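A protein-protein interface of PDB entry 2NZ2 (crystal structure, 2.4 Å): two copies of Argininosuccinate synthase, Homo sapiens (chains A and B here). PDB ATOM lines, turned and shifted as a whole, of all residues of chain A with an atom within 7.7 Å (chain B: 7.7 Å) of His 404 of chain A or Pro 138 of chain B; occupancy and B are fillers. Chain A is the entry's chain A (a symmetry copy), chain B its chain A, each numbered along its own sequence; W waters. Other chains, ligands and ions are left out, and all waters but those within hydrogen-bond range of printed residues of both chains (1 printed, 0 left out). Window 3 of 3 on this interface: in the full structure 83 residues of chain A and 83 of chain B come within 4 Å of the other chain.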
ATOM      1  N   SER A 397     -20.749  33.581  22.855  1.00  0.00           N
ATOM      2  CA  SER A 397     -20.980  32.224  23.390  1.00  0.00           C
ATOM      3  C   SER A 397     -19.707  31.348  23.470  1.00  0.00           C
ATOM      4  O   SER A 397     -19.604  30.449  24.307  1.00  0.00           O
ATOM      5  CB  SER A 397     -22.064  31.497  22.590  1.00  0.00           C
ATOM      6  OG  SER A 397     -21.520  30.823  21.465  1.00  0.00           O
ATOM      7  N   LEU A 398     -18.749  31.605  22.586  1.00  0.00           N
ATOM      8  CA  LEU A 398     -17.499  30.854  22.602  1.00  0.00           C
ATOM      9  C   LEU A 398     -16.917  30.700  24.034  1.00  0.00           C
ATOM     10  O   LEU A 398     -16.706  29.564  24.442  1.00  0.00           O
ATOM     11  CB  LEU A 398     -16.509  31.391  21.540  1.00  0.00           C
ATOM     12  CG  LEU A 398     -14.972  31.288  21.572  1.00  0.00           C
ATOM     13  CD1 LEU A 398     -14.434  29.975  22.134  1.00  0.00           C
ATOM     14  CD2 LEU A 398     -14.362  31.584  20.190  1.00  0.00           C
ATOM     15  N   ARG A 399     -16.708  31.789  24.783  1.00  0.00           N
ATOM     16  CA  ARG A 399     -16.328  31.717  26.233  1.00  0.00           C
ATOM     17  C   ARG A 399     -16.970  30.510  26.936  1.00  0.00           C
ATOM     18  O   ARG A 399     -16.316  29.844  27.717  1.00  0.00           O
ATOM     19  CB  ARG A 399     -16.443  33.056  26.985  1.00  0.00           C
ATOM     20  CG  ARG A 399     -15.395  33.239  28.122  1.00  0.00           C
ATOM     21  CD  ARG A 399     -15.284  34.723  28.607  1.00  0.00           C
ATOM     22  NE  ARG A 399     -16.559  35.437  28.484  1.00  0.00           N
ATOM     23  CZ  ARG A 399     -17.519  35.474  29.405  1.00  0.00           C
ATOM     24  NH1 ARG A 399     -17.368  34.852  30.573  1.00  0.00           N
ATOM     25  NH2 ARG A 399     -18.643  36.134  29.161  1.00  0.00           N
ATOM     26  N   LEU A 400     -18.233  30.188  26.721  1.00  0.00           N
ATOM     27  CA  LEU A 400     -19.370  30.223  27.616  1.00  0.00           C
ATOM     28  C   LEU A 400     -19.567  28.690  27.397  1.00  0.00           C
ATOM     29  O   LEU A 400     -19.633  27.897  28.338  1.00  0.00           O
ATOM     30  CB  LEU A 400     -20.605  30.928  27.080  1.00  0.00           C
ATOM     31  CG  LEU A 400     -21.035  32.227  27.761  1.00  0.00           C
ATOM     32  CD1 LEU A 400     -22.576  32.315  27.742  1.00  0.00           C
ATOM     33  CD2 LEU A 400     -20.459  32.402  29.183  1.00  0.00           C
ATOM     34  N   LYS A 401     -19.602  28.313  26.115  1.00  0.00           N
ATOM     35  CA  LYS A 401     -19.376  26.950  25.644  1.00  0.00           C
ATOM     36  C   LYS A 401     -17.988  26.390  25.960  1.00  0.00           C
ATOM     37  O   LYS A 401     -17.853  25.184  26.136  1.00  0.00           O
ATOM     38  CB  LYS A 401     -19.562  26.859  24.127  1.00  0.00           C
ATOM     39  CG  LYS A 401     -20.931  27.266  23.614  1.00  0.00           C
ATOM     40  CD  LYS A 401     -21.067  26.862  22.143  1.00  0.00           C
ATOM     41  CE  LYS A 401     -20.138  27.679  21.256  1.00  0.00           C
ATOM     42  NZ  LYS A 401     -20.814  27.977  19.958  1.00  0.00           N
ATOM     43  N   GLU A 402     -16.949  27.225  26.024  1.00  0.00           N
ATOM     44  CA  GLU A 402     -15.651  26.667  26.469  1.00  0.00           C
ATOM     45  C   GLU A 402     -15.825  26.048  27.864  1.00  0.00           C
ATOM     46  O   GLU A 402     -15.206  25.017  28.149  1.00  0.00           O
ATOM     47  CB  GLU A 402     -14.418  27.513  26.146  1.00  0.00           C
ATOM     48  CG  GLU A 402     -14.059  27.431  24.649  1.00  0.00           C
ATOM     49  CD  GLU A 402     -13.313  26.134  24.264  1.00  0.00           C
ATOM     50  OE1 GLU A 402     -13.839  25.305  23.480  1.00  0.00           O
ATOM     51  OE2 GLU A 402     -12.175  25.941  24.745  1.00  0.00           O
ATOM     52  N   TYR A 403     -16.615  26.632  28.767  1.00  0.00           N
ATOM     53  CA  TYR A 403     -16.204  27.003  30.088  1.00  0.00           C
ATOM     54  C   TYR A 403     -17.033  25.795  30.611  1.00  0.00           C
ATOM     55  O   TYR A 403     -16.738  25.212  31.639  1.00  0.00           O
ATOM     56  CB  TYR A 403     -16.855  28.237  30.735  1.00  0.00           C
ATOM     57  CG  TYR A 403     -16.771  28.107  32.271  1.00  0.00           C
ATOM     58  CD1 TYR A 403     -15.635  28.564  32.984  1.00  0.00           C
ATOM     59  CD2 TYR A 403     -17.786  27.466  33.010  1.00  0.00           C
ATOM     60  CE1 TYR A 403     -15.536  28.408  34.399  1.00  0.00           C
ATOM     61  CE2 TYR A 403     -17.694  27.318  34.404  1.00  0.00           C
ATOM     62  CZ  TYR A 403     -16.559  27.784  35.086  1.00  0.00           C
ATOM     63  OH  TYR A 403     -16.456  27.613  36.458  1.00  0.00           O
ATOM     64  N   HIS A 404     -18.098  25.461  29.869  1.00  0.00           N
ATOM     65  CA  HIS A 404     -18.982  24.331  30.141  1.00  0.00           C
ATOM     66  C   HIS A 404     -18.285  23.002  29.836  1.00  0.00           C
ATOM     67  O   HIS A 404     -18.266  22.108  30.667  1.00  0.00           O
ATOM     68  CB  HIS A 404     -20.295  24.480  29.338  1.00  0.00           C
ATOM     69  CG  HIS A 404     -21.277  23.370  29.552  1.00  0.00           C
ATOM     70  ND1 HIS A 404     -21.324  22.246  28.753  1.00  0.00           N
ATOM     71  CD2 HIS A 404     -22.250  23.206  30.479  1.00  0.00           C
ATOM     72  CE1 HIS A 404     -22.282  21.441  29.174  1.00  0.00           C
ATOM     73  NE2 HIS A 404     -22.853  21.996  30.227  1.00  0.00           N
ATOM     74  N   ARG A 405     -17.696  22.895  28.644  1.00  0.00           N
ATOM     75  CA  ARG A 405     -16.961  21.705  28.225  1.00  0.00           C
ATOM     76  C   ARG A 405     -15.796  21.384  29.183  1.00  0.00           C
ATOM     77  O   ARG A 405     -15.465  20.216  29.402  1.00  0.00           O
ATOM     78  CB  ARG A 405     -16.453  21.887  26.794  1.00  0.00           C
ATOM     79  CG  ARG A 405     -15.721  20.667  26.220  1.00  0.00           C
ATOM     80  CD  ARG A 405     -15.266  20.865  24.772  1.00  0.00           C
ATOM     81  NE  ARG A 405     -14.329  21.978  24.649  1.00  0.00           N
ATOM     82  CZ  ARG A 405     -13.049  21.909  24.990  1.00  0.00           C
ATOM     83  NH1 ARG A 405     -12.544  20.787  25.472  1.00  0.00           N
ATOM     84  NH2 ARG A 405     -12.268  22.967  24.864  1.00  0.00           N
ATOM     85  N   LEU A 406     -15.199  22.432  29.750  1.00  0.00           N
ATOM     86  CA  LEU A 406     -13.953  22.320  30.501  1.00  0.00           C
ATOM     87  C   LEU A 406     -14.132  22.261  32.015  1.00  0.00           C
ATOM     88  O   LEU A 406     -13.154  22.099  32.737  1.00  0.00           O
ATOM     89  CB  LEU A 406     -12.974  23.446  30.122  1.00  0.00           C
ATOM     90  CG  LEU A 406     -12.289  23.317  28.757  1.00  0.00           C
ATOM     91  CD1 LEU A 406     -11.304  24.458  28.518  1.00  0.00           C
ATOM     92  CD2 LEU A 406     -11.594  21.949  28.613  1.00  0.00           C
ATOM     93  N   GLN A 407     -15.364  22.442  32.491  1.00  0.00           N
ATOM     94  CA  GLN A 407     -15.737  21.969  33.820  1.00  0.00           C
ATOM     95  C   GLN A 407     -16.738  20.794  33.751  1.00  0.00           C
ATOM     96  O   GLN A 407     -17.510  20.575  34.687  1.00  0.00           O
ATOM     97  CB  GLN A 407     -16.203  23.105  34.760  1.00  0.00           C
ATOM     98  CG  GLN A 407     -17.382  23.947  34.299  1.00  0.00           C
ATOM     99  CD  GLN A 407     -18.767  23.323  34.513  1.00  0.00           C
ATOM    100  OE1 GLN A 407     -19.079  22.263  33.965  1.00  0.00           O
ATOM    101  NE2 GLN A 407     -19.626  24.025  35.263  1.00  0.00           N
ATOM    102  N   SER A 408     -16.690  20.022  32.663  1.00  0.00           N
ATOM    103  CA  SER A 408     -17.668  18.952  32.420  1.00  0.00           C
ATOM    104  C   SER A 408     -17.183  17.619  32.949  1.00  0.00           C
ATOM    105  O   SER A 408     -17.358  16.588  32.293  1.00  0.00           O
ATOM    106  CB  SER A 408     -17.979  18.828  30.918  1.00  0.00           C
ATOM    107  OG  SER A 408     -19.218  18.179  30.689  1.00  0.00           O
ATOM    108  N   VAL B 104     -33.927  23.957  26.228  1.00  0.00           N
ATOM    109  CA  VAL B 104     -32.759  23.058  26.124  1.00  0.00           C
ATOM    110  C   VAL B 104     -33.058  21.678  26.768  1.00  0.00           C
ATOM    111  O   VAL B 104     -32.729  20.639  26.198  1.00  0.00           O
ATOM    112  CB  VAL B 104     -31.521  23.742  26.779  1.00  0.00           C
ATOM    113  CG1 VAL B 104     -30.399  22.776  27.123  1.00  0.00           C
ATOM    114  CG2 VAL B 104     -31.027  24.850  25.893  1.00  0.00           C
ATOM    115  N   GLN B 108     -33.051  18.176  24.634  1.00  0.00           N
ATOM    116  CA  GLN B 108     -32.113  17.090  24.904  1.00  0.00           C
ATOM    117  C   GLN B 108     -32.859  15.837  25.278  1.00  0.00           C
ATOM    118  O   GLN B 108     -32.396  14.724  24.998  1.00  0.00           O
ATOM    119  CB  GLN B 108     -31.129  17.480  25.990  1.00  0.00           C
ATOM    120  CG  GLN B 108     -30.254  18.632  25.569  1.00  0.00           C
ATOM    121  CD  GLN B 108     -29.176  18.906  26.564  1.00  0.00           C
ATOM    122  OE1 GLN B 108     -29.425  18.930  27.767  1.00  0.00           O
ATOM    123  NE2 GLN B 108     -27.953  19.106  26.074  1.00  0.00           N
ATOM    124  N   SER B 132     -27.885  31.309  26.699  1.00  0.00           N
ATOM    125  CA  SER B 132     -28.263  30.234  27.654  1.00  0.00           C
ATOM    126  C   SER B 132     -28.288  28.852  27.007  1.00  0.00           C
ATOM    127  O   SER B 132     -27.890  27.865  27.624  1.00  0.00           O
ATOM    128  CB  SER B 132     -29.641  30.497  28.297  1.00  0.00           C
ATOM    129  OG  SER B 132     -29.572  31.524  29.267  1.00  0.00           O
ATOM    130  N   CYS B 133     -28.784  28.777  25.776  1.00  0.00           N
ATOM    131  CA  CYS B 133     -28.815  27.510  25.036  1.00  0.00           C
ATOM    132  C   CYS B 133     -27.411  26.948  24.801  1.00  0.00           C
ATOM    133  O   CYS B 133     -27.146  25.798  25.128  1.00  0.00           O
ATOM    134  CB  CYS B 133     -29.531  27.691  23.708  1.00  0.00           C
ATOM    135  SG  CYS B 133     -31.299  27.896  23.880  1.00  0.00           S
ATOM    136  N   TYR B 134     -26.521  27.776  24.245  1.00  0.00           N
ATOM    137  CA  TYR B 134     -25.134  27.395  24.033  1.00  0.00           C
ATOM    138  C   TYR B 134     -24.416  27.132  25.361  1.00  0.00           C
ATOM    139  O   TYR B 134     -23.671  26.188  25.480  1.00  0.00           O
ATOM    140  CB  TYR B 134     -24.392  28.474  23.245  1.00  0.00           C
ATOM    141  CG  TYR B 134     -24.842  28.638  21.816  1.00  0.00           C
ATOM    142  CD1 TYR B 134     -25.007  27.522  20.983  1.00  0.00           C
ATOM    143  CD2 TYR B 134     -25.083  29.902  21.284  1.00  0.00           C
ATOM    144  CE1 TYR B 134     -25.426  27.655  19.651  1.00  0.00           C
ATOM    145  CE2 TYR B 134     -25.488  30.066  19.933  1.00  0.00           C
ATOM    146  CZ  TYR B 134     -25.666  28.920  19.128  1.00  0.00           C
ATOM    147  OH  TYR B 134     -26.063  29.031  17.805  1.00  0.00           O
ATOM    148  N   SER B 135     -24.653  27.974  26.362  1.00  0.00           N
ATOM    149  CA  SER B 135     -23.980  27.805  27.637  1.00  0.00           C
ATOM    150  C   SER B 135     -24.337  26.475  28.268  1.00  0.00           C
ATOM    151  O   SER B 135     -23.478  25.801  28.797  1.00  0.00           O
ATOM    152  CB  SER B 135     -24.315  28.944  28.617  1.00  0.00           C
ATOM    153  OG  SER B 135     -23.542  28.805  29.803  1.00  0.00           O
ATOM    154  N   LEU B 136     -25.613  26.104  28.194  1.00  0.00           N
ATOM    155  CA  LEU B 136     -26.113  24.877  28.819  1.00  0.00           C
ATOM    156  C   LEU B 136     -25.943  23.649  27.944  1.00  0.00           C
ATOM    157  O   LEU B 136     -25.803  22.541  28.447  1.00  0.00           O
ATOM    158  CB  LEU B 136     -27.580  25.060  29.217  1.00  0.00           C
ATOM    159  CG  LEU B 136     -27.829  26.120  30.303  1.00  0.00           C
ATOM    160  CD1 LEU B 136     -29.271  26.605  30.277  1.00  0.00           C
ATOM    161  CD2 LEU B 136     -27.451  25.604  31.695  1.00  0.00           C
ATOM    162  N   ALA B 137     -25.948  23.856  26.629  1.00  0.00           N
ATOM    163  CA  ALA B 137     -25.774  22.785  25.648  1.00  0.00           C
ATOM    164  C   ALA B 137     -24.950  23.296  24.487  1.00  0.00           C
ATOM    165  O   ALA B 137     -25.503  23.757  23.489  1.00  0.00           O
ATOM    166  CB  ALA B 137     -27.143  22.266  25.167  1.00  0.00           C
ATOM    167  N   PRO B 138     -23.619  23.248  24.616  1.00  0.00           N
ATOM    168  CA  PRO B 138     -22.712  23.767  23.570  1.00  0.00           C
ATOM    169  C   PRO B 138     -22.941  23.216  22.150  1.00  0.00           C
ATOM    170  O   PRO B 138     -22.656  23.902  21.169  1.00  0.00           O
ATOM    171  CB  PRO B 138     -21.315  23.373  24.085  1.00  0.00           C
ATOM    172  CG  PRO B 138     -21.501  23.294  25.601  1.00  0.00           C
ATOM    173  CD  PRO B 138     -22.882  22.729  25.782  1.00  0.00           C
ATOM    174  N   GLN B 139     -23.463  22.004  22.036  1.00  0.00           N
ATOM    175  CA  GLN B 139     -23.676  21.422  20.725  1.00  0.00           C
ATOM    176  C   GLN B 139     -25.033  21.705  20.069  1.00  0.00           C
ATOM    177  O   GLN B 139     -25.209  21.313  18.902  1.00  0.00           O
ATOM    178  CB  GLN B 139     -23.442  19.905  20.745  1.00  0.00           C
ATOM    179  CG  GLN B 139     -22.092  19.437  21.247  1.00  0.00           C
ATOM    180  CD  GLN B 139     -22.104  17.932  21.459  1.00  0.00           C
ATOM    181  OE1 GLN B 139     -23.168  17.283  21.351  1.00  0.00           O
ATOM    182  NE2 GLN B 139     -20.927  17.353  21.763  1.00  0.00           N
ATOM    183  N   ILE B 140     -25.987  22.347  20.759  1.00  0.00           N
ATOM    184  CA  ILE B 140     -27.287  22.613  20.069  1.00  0.00           C
ATOM    185  C   ILE B 140     -27.120  23.596  18.932  1.00  0.00           C
ATOM    186  O   ILE B 140     -26.180  24.388  18.902  1.00  0.00           O
ATOM    187  CB  ILE B 140     -28.507  23.113  20.949  1.00  0.00           C
ATOM    188  CG1 ILE B 140     -28.071  24.084  22.039  1.00  0.00           C
ATOM    189  CG2 ILE B 140     -29.420  21.989  21.395  1.00  0.00           C
ATOM    190  CD1 ILE B 140     -27.835  25.478  21.476  1.00  0.00           C
ATOM    191  N   LYS B 141     -28.046  23.540  17.997  1.00  0.00           N
ATOM    192  CA  LYS B 141     -28.022  24.445  16.872  1.00  0.00           C
ATOM    193  C   LYS B 141     -29.230  25.349  17.003  1.00  0.00           C
ATOM    194  O   LYS B 141     -30.292  24.919  17.477  1.00  0.00           O
ATOM    195  CB  LYS B 141     -28.030  23.662  15.548  1.00  0.00           C
ATOM    196  CG  LYS B 141     -26.684  23.036  15.198  1.00  0.00           C
ATOM    197  CD  LYS B 141     -26.820  22.000  14.090  1.00  0.00           C
ATOM    198  CE  LYS B 141     -26.705  20.599  14.642  1.00  0.00           C
ATOM    199  NZ  LYS B 141     -26.843  19.544  13.591  1.00  0.00           N
ATOM    200  N   PRO B 330     -20.056  31.695  34.006  1.00  0.00           N
ATOM    201  CA  PRO B 330     -19.313  31.662  35.260  1.00  0.00           C
ATOM    202  C   PRO B 330     -19.360  33.001  36.013  1.00  0.00           C
ATOM    203  O   PRO B 330     -19.454  32.989  37.239  1.00  0.00           O
ATOM    204  CB  PRO B 330     -17.890  31.306  34.824  1.00  0.00           C
ATOM    205  CG  PRO B 330     -17.881  31.428  33.353  1.00  0.00           C
ATOM    206  CD  PRO B 330     -19.232  31.294  32.853  1.00  0.00           C
HETATM  207  O   HOH W   1     -20.986  28.133  30.323  1.00  0.00           O
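NE2 of His 404 of chain A lies within hydrogen-bond range of O of Leu 136 of chain B.
The side-chain amino group of Lys 401 of chain A is in hydrogen-bond range of the side-chain hydroxyl of Ser 397 of chain A (3.3 Å). The backbone carbonyl oxygen of His 404 of chain A lies close to the side-chain amide oxygen of Gln 407 of chain A (3.4 Å).
Among the printed residues, merely in contact across the chains: His 404 of chain A with Pro 138 of chain B (3.3 Å), His 404 of chain A with Ser 135 of chain B (3.3 Å), Lys 401 of chain A with Tyr 134 of chain B (3.5 Å), Lys 401 of chain A with Pro 138 of chain B (3.5 Å), Ser 397 of chain A with Tyr 134 of chain B (3.7 Å), Tyr 403 of chain A with Pro 330 of chain B (3.7 Å) and Leu 400 of chain A with Ser 135 of chain B (3.9 Å).
Of chain B, only Ser 135 (3.3 Å), Leu 136 (3.5 Å) and Pro 138 (3.3 Å) come within 4 Å of His 404 of chain A. Pro 138 of chain B touches just these residues of chain A: Lys 401 and His 404. Printed residues of chain A within 4 Å of Pro 330 of chain B: Tyr 403 (3.7 Å). Of the printed residues of chain A, Ser 135 of chain B touches Leu 400 (3.9 Å) and His 404 (3.3 Å). Val 104 of chain B touches none of the printed residues of chain A. The nearest residue of chain B that does not touch His 404 of chain A is Ala 137 of chain B (5.1 Å). The nearest residue of chain A that does not touch Pro 138 of chain B is Arg 405 of chain A (4.9 Å). The nearest printed residue of chain A that does not touch Pro 330 of chain B is Leu 400 of chain A (4.03 Å).
Hydrophobic or aromatic side chains of chain A that line the printed part of chain B: Leu 400, Tyr 403 and His 404. Among the printed residues, 8 pairs touch across the chains.
No position is printed for both chains. Of the 8 pairs that touch across the chains among the printed residues, none has its exchanged pair printed and touching as well.
Water W1 bridges O of Leu 400 of chain A (2.4 Å) and OG of Ser 135 of chain B (2.7 Å).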
